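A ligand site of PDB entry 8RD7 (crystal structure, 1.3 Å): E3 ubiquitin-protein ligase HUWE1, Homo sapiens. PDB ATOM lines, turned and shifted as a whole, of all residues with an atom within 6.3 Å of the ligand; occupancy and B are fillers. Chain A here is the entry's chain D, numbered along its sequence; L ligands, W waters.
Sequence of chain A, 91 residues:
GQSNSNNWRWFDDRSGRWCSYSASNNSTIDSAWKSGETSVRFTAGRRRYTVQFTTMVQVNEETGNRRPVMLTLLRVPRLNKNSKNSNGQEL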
ATOM      1  N   TRP A  10     -22.534  27.776 -31.934  1.00  0.00           N
ATOM      2  CA  TRP A  10     -23.767  27.788 -31.161  1.00  0.00           C
ATOM      3  C   TRP A  10     -23.751  29.008 -30.231  1.00  0.00           C
ATOM      4  O   TRP A  10     -22.689  29.418 -29.738  1.00  0.00           O
ATOM      5  CB  TRP A  10     -23.918  26.474 -30.339  1.00  0.00           C
ATOM      6  CG  TRP A  10     -22.800  26.242 -29.403  1.00  0.00           C
ATOM      7  CD1 TRP A  10     -21.552  25.711 -29.689  1.00  0.00           C
ATOM      8  CD2 TRP A  10     -22.810  26.459 -27.987  1.00  0.00           C
ATOM      9  NE1 TRP A  10     -20.784  25.628 -28.546  1.00  0.00           N
ATOM     10  CE2 TRP A  10     -21.537  26.083 -27.484  1.00  0.00           C
ATOM     11  CE3 TRP A  10     -23.774  26.962 -27.083  1.00  0.00           C
ATOM     12  CZ2 TRP A  10     -21.191  26.199 -26.129  1.00  0.00           C
ATOM     13  CZ3 TRP A  10     -23.446  27.069 -25.720  1.00  0.00           C
ATOM     14  CH2 TRP A  10     -22.161  26.680 -25.265  1.00  0.00           C
ATOM     15  N   ASP A  12     -24.229  31.065 -26.865  1.00  0.00           N
ATOM     16  CA  ASP A  12     -24.267  30.887 -25.412  1.00  0.00           C
ATOM     17  C   ASP A  12     -24.884  32.143 -24.782  1.00  0.00           C
ATOM     18  O   ASP A  12     -24.223  33.173 -24.645  1.00  0.00           O
ATOM     19  CB  ASP A  12     -22.840  30.639 -24.913  1.00  0.00           C
ATOM     20  CG  ASP A  12     -22.773  30.341 -23.432  1.00  0.00           C
ATOM     21  OD1 ASP A  12     -23.764  30.532 -22.694  1.00  0.00           O
ATOM     22  OD2 ASP A  12     -21.710  29.857 -22.994  1.00  0.00           O
ATOM     23  N   ARG A  14     -25.482  32.742 -21.752  1.00  0.00           N
ATOM     24  CA  ARG A  14     -24.897  33.135 -20.478  1.00  0.00           C
ATOM     25  C   ARG A  14     -23.744  34.088 -20.684  1.00  0.00           C
ATOM     26  O   ARG A  14     -23.514  34.993 -19.851  1.00  0.00           O
ATOM     27  CB  ARG A  14     -24.350  31.924 -19.746  1.00  0.00           C
ATOM     28  CG  ARG A  14     -25.368  30.903 -19.404  1.00  0.00           C
ATOM     29  CD  ARG A  14     -26.353  31.316 -18.304  1.00  0.00           C
ATOM     30  NE  ARG A  14     -27.218  30.181 -17.940  1.00  0.00           N
ATOM     31  CZ  ARG A  14     -28.306  30.300 -17.187  1.00  0.00           C
ATOM     32  NH1 ARG A  14     -28.674  31.474 -16.708  1.00  0.00           N
ATOM     33  NH2 ARG A  14     -29.043  29.204 -16.927  1.00  0.00           N
ATOM     34  N   SER A  20     -17.572  28.416 -30.663  1.00  0.00           N
ATOM     35  CA  SER A  20     -17.222  27.418 -31.665  1.00  0.00           C
ATOM     36  C   SER A  20     -17.547  26.039 -31.101  1.00  0.00           C
ATOM     37  O   SER A  20     -17.429  25.800 -29.907  1.00  0.00           O
ATOM     38  CB  SER A  20     -15.718  27.459 -31.935  1.00  0.00           C
ATOM     39  OG  SER A  20     -15.398  28.651 -32.629  1.00  0.00           O
ATOM     40  N   TYR A  21     -17.900  25.110 -31.987  1.00  0.00           N
ATOM     41  CA  TYR A  21     -17.958  23.720 -31.563  1.00  0.00           C
ATOM     42  C   TYR A  21     -16.544  23.153 -31.480  1.00  0.00           C
ATOM     43  O   TYR A  21     -15.595  23.685 -32.066  1.00  0.00           O
ATOM     44  CB  TYR A  21     -18.767  22.904 -32.555  1.00  0.00           C
ATOM     45  CG  TYR A  21     -20.263  23.041 -32.397  1.00  0.00           C
ATOM     46  CD1 TYR A  21     -20.933  22.253 -31.469  1.00  0.00           C
ATOM     47  CD2 TYR A  21     -21.007  23.931 -33.164  1.00  0.00           C
ATOM     48  CE1 TYR A  21     -22.283  22.329 -31.293  1.00  0.00           C
ATOM     49  CE2 TYR A  21     -22.389  24.058 -32.988  1.00  0.00           C
ATOM     50  CZ  TYR A  21     -23.038  23.246 -32.052  1.00  0.00           C
ATOM     51  OH  TYR A  21     -24.397  23.348 -31.891  1.00  0.00           O
ATOM     52  N   SER A  22     -16.407  22.059 -30.728  1.00  0.00           N
ATOM     53  CA  SER A  22     -15.143  21.348 -30.703  1.00  0.00           C
ATOM     54  C   SER A  22     -14.824  20.854 -32.098  1.00  0.00           C
ATOM     55  O   SER A  22     -15.701  20.733 -32.961  1.00  0.00           O
ATOM     56  CB  SER A  22     -15.227  20.135 -29.769  1.00  0.00           C
ATOM     57  OG  SER A  22     -16.125  19.175 -30.274  1.00  0.00           O
ATOM     58  N   ASN A  25     -16.872  17.818 -32.867  1.00  0.00           N
ATOM     59  CA  ASN A  25     -18.288  18.073 -33.047  1.00  0.00           C
ATOM     60  C   ASN A  25     -18.522  18.871 -34.307  1.00  0.00           C
ATOM     61  O   ASN A  25     -19.476  18.604 -35.042  1.00  0.00           O
ATOM     62  CB  ASN A  25     -18.897  18.751 -31.823  1.00  0.00           C
ATOM     63  CG  ASN A  25     -19.078  17.778 -30.686  1.00  0.00           C
ATOM     64  OD1 ASN A  25     -19.146  16.559 -30.896  1.00  0.00           O
ATOM     65  ND2 ASN A  25     -19.149  18.313 -29.462  1.00  0.00           N
ATOM     66  N   PHE A  42     -24.849  14.678 -31.512  1.00  0.00           N
ATOM     67  CA  PHE A  42     -23.514  14.790 -30.968  1.00  0.00           C
ATOM     68  C   PHE A  42     -23.612  14.800 -29.449  1.00  0.00           C
ATOM     69  O   PHE A  42     -24.716  14.853 -28.874  1.00  0.00           O
ATOM     70  CB  PHE A  42     -22.782  16.009 -31.545  1.00  0.00           C
ATOM     71  CG  PHE A  42     -23.276  17.355 -31.009  1.00  0.00           C
ATOM     72  CD1 PHE A  42     -24.305  18.080 -31.623  1.00  0.00           C
ATOM     73  CD2 PHE A  42     -22.695  17.894 -29.873  1.00  0.00           C
ATOM     74  CE1 PHE A  42     -24.701  19.300 -31.117  1.00  0.00           C
ATOM     75  CE2 PHE A  42     -23.146  19.116 -29.344  1.00  0.00           C
ATOM     76  CZ  PHE A  42     -24.131  19.806 -29.971  1.00  0.00           C
ATOM     77  N   ALA A  44     -21.590  16.719 -25.963  1.00  0.00           N
ATOM     78  CA  ALA A  44     -20.605  17.670 -25.428  1.00  0.00           C
ATOM     79  C   ALA A  44     -20.730  17.757 -23.919  1.00  0.00           C
ATOM     80  O   ALA A  44     -21.844  17.837 -23.396  1.00  0.00           O
ATOM     81  CB  ALA A  44     -20.768  19.075 -26.036  1.00  0.00           C
ATOM     82  N   GLY A  45     -19.609  17.636 -23.209  1.00  0.00           N
ATOM     83  CA  GLY A  45     -19.678  17.706 -21.762  1.00  0.00           C
ATOM     84  C   GLY A  45     -20.538  16.616 -21.157  1.00  0.00           C
ATOM     85  O   GLY A  45     -21.185  16.845 -20.124  1.00  0.00           O
ATOM     86  N   ARG A  47     -23.292  15.548 -22.244  1.00  0.00           N
ATOM     87  CA  ARG A  47     -24.698  15.795 -22.521  1.00  0.00           C
ATOM     88  C   ARG A  47     -24.971  15.462 -23.971  1.00  0.00           C
ATOM     89  O   ARG A  47     -24.110  15.681 -24.831  1.00  0.00           O
ATOM     90  CB  ARG A  47     -25.067  17.281 -22.265  1.00  0.00           C
ATOM     91  CG  ARG A  47     -24.785  17.696 -20.836  1.00  0.00           C
ATOM     92  CD  ARG A  47     -25.413  19.052 -20.526  1.00  0.00           C
ATOM     93  NE  ARG A  47     -25.223  19.466 -19.136  1.00  0.00           N
ATOM     94  CZ  ARG A  47     -24.108  19.997 -18.663  1.00  0.00           C
ATOM     95  NH1 ARG A  47     -23.099  20.303 -19.475  1.00  0.00           N
ATOM     96  NH2 ARG A  47     -23.994  20.228 -17.341  1.00  0.00           N
ATOM     97  N   TYR A  49     -27.041  15.933 -27.471  1.00  0.00           N
ATOM     98  CA  TYR A  49     -27.698  16.996 -28.231  1.00  0.00           C
ATOM     99  C   TYR A  49     -28.089  16.538 -29.617  1.00  0.00           C
ATOM    100  O   TYR A  49     -27.426  15.684 -30.220  1.00  0.00           O
ATOM    101  CB  TYR A  49     -26.720  18.166 -28.480  1.00  0.00           C
ATOM    102  CG  TYR A  49     -26.282  18.834 -27.228  1.00  0.00           C
ATOM    103  CD1 TYR A  49     -27.046  19.834 -26.663  1.00  0.00           C
ATOM    104  CD2 TYR A  49     -25.103  18.453 -26.575  1.00  0.00           C
ATOM    105  CE1 TYR A  49     -26.667  20.481 -25.486  1.00  0.00           C
ATOM    106  CE2 TYR A  49     -24.703  19.091 -25.432  1.00  0.00           C
ATOM    107  CZ  TYR A  49     -25.481  20.108 -24.869  1.00  0.00           C
ATOM    108  OH  TYR A  49     -25.065  20.712 -23.691  1.00  0.00           O
ATOM    109  N   GLN A  58     -29.662  23.774 -31.746  1.00  0.00           N
ATOM    110  CA  GLN A  58     -29.219  22.576 -31.041  1.00  0.00           C
ATOM    111  C   GLN A  58     -30.118  22.373 -29.839  1.00  0.00           C
ATOM    112  O   GLN A  58     -30.503  23.347 -29.171  1.00  0.00           O
ATOM    113  CB  GLN A  58     -27.759  22.657 -30.629  1.00  0.00           C
ATOM    114  CG  GLN A  58     -27.378  23.751 -29.723  1.00  0.00           C
ATOM    115  CD  GLN A  58     -26.205  23.291 -28.801  1.00  0.00           C
ATOM    116  OE1 GLN A  58     -25.071  23.003 -29.258  1.00  0.00           O
ATOM    117  NE2 GLN A  58     -26.469  23.301 -27.507  1.00  0.00           N
ATOM    118  N   ASN A  60     -30.828  20.246 -26.301  1.00  0.00           N
ATOM    119  CA  ASN A  60     -30.455  19.312 -25.238  1.00  0.00           C
ATOM    120  C   ASN A  60     -31.545  18.245 -25.142  1.00  0.00           C
ATOM    121  O   ASN A  60     -32.723  18.580 -24.961  1.00  0.00           O
ATOM    122  CB  ASN A  60     -30.257  20.069 -23.928  1.00  0.00           C
ATOM    123  CG  ASN A  60     -29.942  19.152 -22.745  1.00  0.00           C
ATOM    124  OD1 ASN A  60     -30.676  18.203 -22.479  1.00  0.00           O
ATOM    125  ND2 ASN A  60     -28.819  19.394 -22.067  1.00  0.00           N
ATOM    126  N   THR A  63     -33.396  18.094 -21.440  1.00  0.00           N
ATOM    127  CA  THR A  63     -34.169  19.228 -20.927  1.00  0.00           C
ATOM    128  C   THR A  63     -35.004  19.900 -21.999  1.00  0.00           C
ATOM    129  O   THR A  63     -35.927  20.666 -21.668  1.00  0.00           O
ATOM    130  CB  THR A  63     -33.244  20.305 -20.345  1.00  0.00           C
ATOM    131  OG1 THR A  63     -32.464  20.896 -21.384  1.00  0.00           O
ATOM    132  CG2 THR A  63     -32.302  19.696 -19.327  1.00  0.00           C
ATOM    133  N   GLY A  64     -34.670  19.673 -23.273  1.00  0.00           N
ATOM    134  CA  GLY A  64     -35.306  20.361 -24.361  1.00  0.00           C
ATOM    135  C   GLY A  64     -34.783  21.761 -24.614  1.00  0.00           C
ATOM    136  O   GLY A  64     -35.292  22.434 -25.512  1.00  0.00           O
ATOM    137  N   ASN A  65     -33.793  22.228 -23.860  1.00  0.00           N
ATOM    138  CA  ASN A  65     -33.294  23.593 -24.073  1.00  0.00           C
ATOM    139  C   ASN A  65     -32.735  23.736 -25.487  1.00  0.00           C
ATOM    140  O   ASN A  65     -31.892  22.929 -25.917  1.00  0.00           O
ATOM    141  CB  ASN A  65     -32.191  23.906 -23.059  1.00  0.00           C
ATOM    142  CG  ASN A  65     -31.805  25.391 -23.044  1.00  0.00           C
ATOM    143  OD1 ASN A  65     -32.681  26.263 -22.917  1.00  0.00           O
ATOM    144  ND2 ASN A  65     -30.517  25.688 -23.191  1.00  0.00           N
ATOM    145  N   ARG A  66     -33.167  24.784 -26.179  1.00  0.00           N
ATOM    146  CA  ARG A  66     -32.791  25.089 -27.544  1.00  0.00           C
ATOM    147  C   ARG A  66     -31.855  26.282 -27.552  1.00  0.00           C
ATOM    148  O   ARG A  66     -32.202  27.355 -27.029  1.00  0.00           O
ATOM    149  CB  ARG A  66     -34.042  25.407 -28.388  1.00  0.00           C
ATOM    150  CG  ARG A  66     -35.019  24.222 -28.555  1.00  0.00           C
ATOM    151  CD  ARG A  66     -36.414  24.631 -29.042  1.00  0.00           C
ATOM    152  NE  ARG A  66     -36.418  25.185 -30.388  1.00  0.00           N
ATOM    153  CZ  ARG A  66     -36.449  24.505 -31.531  1.00  0.00           C
ATOM    154  NH1 ARG A  66     -36.462  23.172 -31.561  1.00  0.00           N
ATOM    155  NH2 ARG A  66     -36.450  25.186 -32.686  1.00  0.00           N
ATOM    156  N   ARG A  67     -30.671  26.094 -28.185  1.00  0.00           N
ATOM    157  CA  ARG A  67     -29.743  27.199 -28.426  1.00  0.00           C
ATOM    158  C   ARG A  67     -29.528  27.298 -29.933  1.00  0.00           C
ATOM    159  O   ARG A  67     -29.415  26.256 -30.628  1.00  0.00           O
ATOM    160  CB  ARG A  67     -28.388  26.934 -27.739  1.00  0.00           C
ATOM    161  CG  ARG A  67     -28.558  26.799 -26.209  1.00  0.00           C
ATOM    162  CD  ARG A  67     -27.220  26.600 -25.558  1.00  0.00           C
ATOM    163  NE  ARG A  67     -27.361  26.299 -24.129  1.00  0.00           N
ATOM    164  CZ  ARG A  67     -27.324  27.206 -23.168  1.00  0.00           C
ATOM    165  NH1 ARG A  67     -27.223  28.512 -23.453  1.00  0.00           N
ATOM    166  NH2 ARG A  67     -27.395  26.800 -21.885  1.00  0.00           N
HETATM  167  N1  LIG L   1     -20.764  22.691 -26.403  1.00  0.00           N
HETATM  168  C1  LIG L   1     -20.347  22.852 -25.143  1.00  0.00           C
HETATM  169  N2  LIG L   1     -21.065  23.206 -24.091  1.00  0.00           N
HETATM  170  C2  LIG L   1     -22.358  23.372 -24.413  1.00  0.00           C
HETATM  171  C3  LIG L   1     -22.942  23.220 -25.678  1.00  0.00           C
HETATM  172  C4  LIG L   1     -22.068  22.855 -26.717  1.00  0.00           C
HETATM  173  N3  LIG L   1     -22.461  22.727 -27.981  1.00  0.00           N
HETATM  174  N4  LIG L   1     -24.294  23.499 -25.629  1.00  0.00           N
HETATM  175  C5  LIG L   1     -24.522  23.788 -24.373  1.00  0.00           C
HETATM  176  N5  LIG L   1     -23.393  23.731 -23.593  1.00  0.00           N
HETATM  177  P1  LIG L   1     -27.815  22.940 -22.198  1.00  0.00           P
HETATM  178  P2  LIG L   1     -29.803  23.442 -20.073  1.00  0.00           P
HETATM  179  C6  LIG L   1     -23.304  23.987 -22.176  1.00  0.00           C
HETATM  180  O1  LIG L   1     -28.275  23.792 -23.309  1.00  0.00           O
HETATM  181  O2  LIG L   1     -31.201  22.880 -20.042  1.00  0.00           O
HETATM  182  C7  LIG L   1     -26.937  22.691 -15.871  1.00  0.00           C
HETATM  183  O3  LIG L   1     -26.579  22.027 -14.689  1.00  0.00           O
HETATM  184  C8  LIG L   1     -23.976  25.296 -21.746  1.00  0.00           C
HETATM  185  O4  LIG L   1     -23.101  26.369 -21.913  1.00  0.00           O
HETATM  186  O5  LIG L   1     -27.211  21.644 -22.581  1.00  0.00           O
HETATM  187  O6  LIG L   1     -29.548  24.887 -20.274  1.00  0.00           O
HETATM  188  C9  LIG L   1     -28.285  23.384 -15.642  1.00  0.00           C
HETATM  189  O7  LIG L   1     -28.492  23.674 -14.272  1.00  0.00           O
HETATM  190  C10 LIG L   1     -24.357  24.965 -20.312  1.00  0.00           C
HETATM  191  O8  LIG L   1     -23.254  25.195 -19.495  1.00  0.00           O
HETATM  192  O9  LIG L   1     -29.019  22.590 -21.179  1.00  0.00           O
HETATM  193  C11 LIG L   1     -29.230  22.228 -15.997  1.00  0.00           C
HETATM  194  O10 LIG L   1     -29.581  21.435 -14.895  1.00  0.00           O
HETATM  195  C12 LIG L   1     -24.593  23.446 -20.317  1.00  0.00           C
HETATM  196  O11 LIG L   1     -23.987  22.952 -21.519  1.00  0.00           O
HETATM  197  C13 LIG L   1     -28.477  21.394 -17.030  1.00  0.00           C
HETATM  198  O12 LIG L   1     -27.116  21.782 -16.951  1.00  0.00           O
HETATM  199  C14 LIG L   1     -26.074  23.083 -20.258  1.00  0.00           C
HETATM  200  O13 LIG L   1     -26.758  23.779 -21.288  1.00  0.00           O
HETATM  201  C15 LIG L   1     -29.023  21.599 -18.427  1.00  0.00           C
HETATM  202  O14 LIG L   1     -28.946  22.979 -18.768  1.00  0.00           O
HETATM  203  O   HOH W   1     -20.216  21.373 -21.537  1.00  0.00           O
HETATM  204  O   HOH W   2     -22.479  27.803 -18.773  1.00  0.00           O
HETATM  205  O   HOH W   3     -20.099  26.251 -21.800  1.00  0.00           O
HETATM  206  O   HOH W   4     -30.821  27.224 -20.116  1.00  0.00           O
HETATM  207  O   HOH W   5     -33.333  24.073 -19.043  1.00  0.00           O
HETATM  208  O   HOH W   6     -24.462  28.537 -21.035  1.00  0.00           O
HETATM  209  O   HOH W   7     -21.349  23.057 -18.683  1.00  0.00           O
HETATM  210  O   HOH W   8     -22.548  20.211 -22.459  1.00  0.00           O
HETATM  211  O   HOH W   9     -28.980  23.316 -26.021  1.00  0.00           O
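O of Phe 42 sits at hydrogen-bond distance from N of Tyr 49 (2.9 Å). OD1 of Asn 60 sits at hydrogen-bond distance from N of Thr 63, 2.9 Å away. The side-chain hydroxyl (OG1) of Thr 63 lies within hydrogen-bond range of the backbone NH (N) of Asn 65, 3.1 Å away. The backbone carbonyl oxygen (O) of Arg 67 lies within hydrogen-bond range of the backbone NH (N) of Gln 58, 2.7 Å away. NE of Arg 67 lies close to ND2 of Asn 65. The backbone carbonyl oxygen (O) of Asn 65 lies within hydrogen-bond range of the backbone NH (N) of Asn 60 (2.9 Å). OE1 of Gln 58 is in hydrogen-bond range of OH of Tyr 21. OD1 of Asp 12 is in hydrogen-bond range of N of Arg 14 (3.0 Å).
Water W4 bridges an oxygen (O6) of the ligand (2.7 Å) and the side-chain amide nitrogen of Asn 65 (3.5 Å). Water W6 lies within hydrogen-bond range of the side-chain carboxylate (OD1) of Asp 12 (2.7 Å) and an oxygen (O4) of the ligand (2.7 Å). Water W9 lies within hydrogen-bond range of an oxygen (O1) of the ligand, the side-chain amide nitrogen (NE2) of Gln 58 and the backbone carbonyl oxygen (O) of Asn 65. Water W7 lies within hydrogen-bond range of O8 of the ligand and NH1 of Arg 47. Water W8 lies within hydrogen-bond range of O of Ala 44, OH of Tyr 49, NH1 of Arg 47 and O11 of the ligand.
OH of Tyr 49 lies within hydrogen-bond range of O5 of the ligand (2.6 Å). O2 of the ligand sits at hydrogen-bond distance from OG1 of Thr 63 (2.7 Å). O1 of the ligand is in salt-bridge range of NE of Arg 67. O5 of the ligand lies within hydrogen-bond range of ND2 of Asn 60. NE2 of Gln 58 is in hydrogen-bond range of N4 of the ligand (2.9 Å). The side-chain amide nitrogen of Asn 65 sits at hydrogen-bond distance from an oxygen (O1) of the ligand. An oxygen (O11) of the ligand lies within hydrogen-bond range of the guanidinium group of Arg 47.
The indole nitrogen (NE1) of Trp 10 sits close to a nitrogen (N3) of the ligand, 3.4 Å away. Merely in contact with the ligand: Tyr 21 (3.3 Å), Ala 44 (3.6 Å), Asp 12 (3.9 Å) and Phe 42 (3.9 Å). Within 4 Å of the ligand: Trp 10, Asp 12, Tyr 21, Phe 42, Ala 44, Arg 47, Tyr 49, Gln 58, Asn 60, Thr 63, Asn 65 and Arg 67. The nearest printed residue that does not touch the ligand is Arg 14 (5.5 Å).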
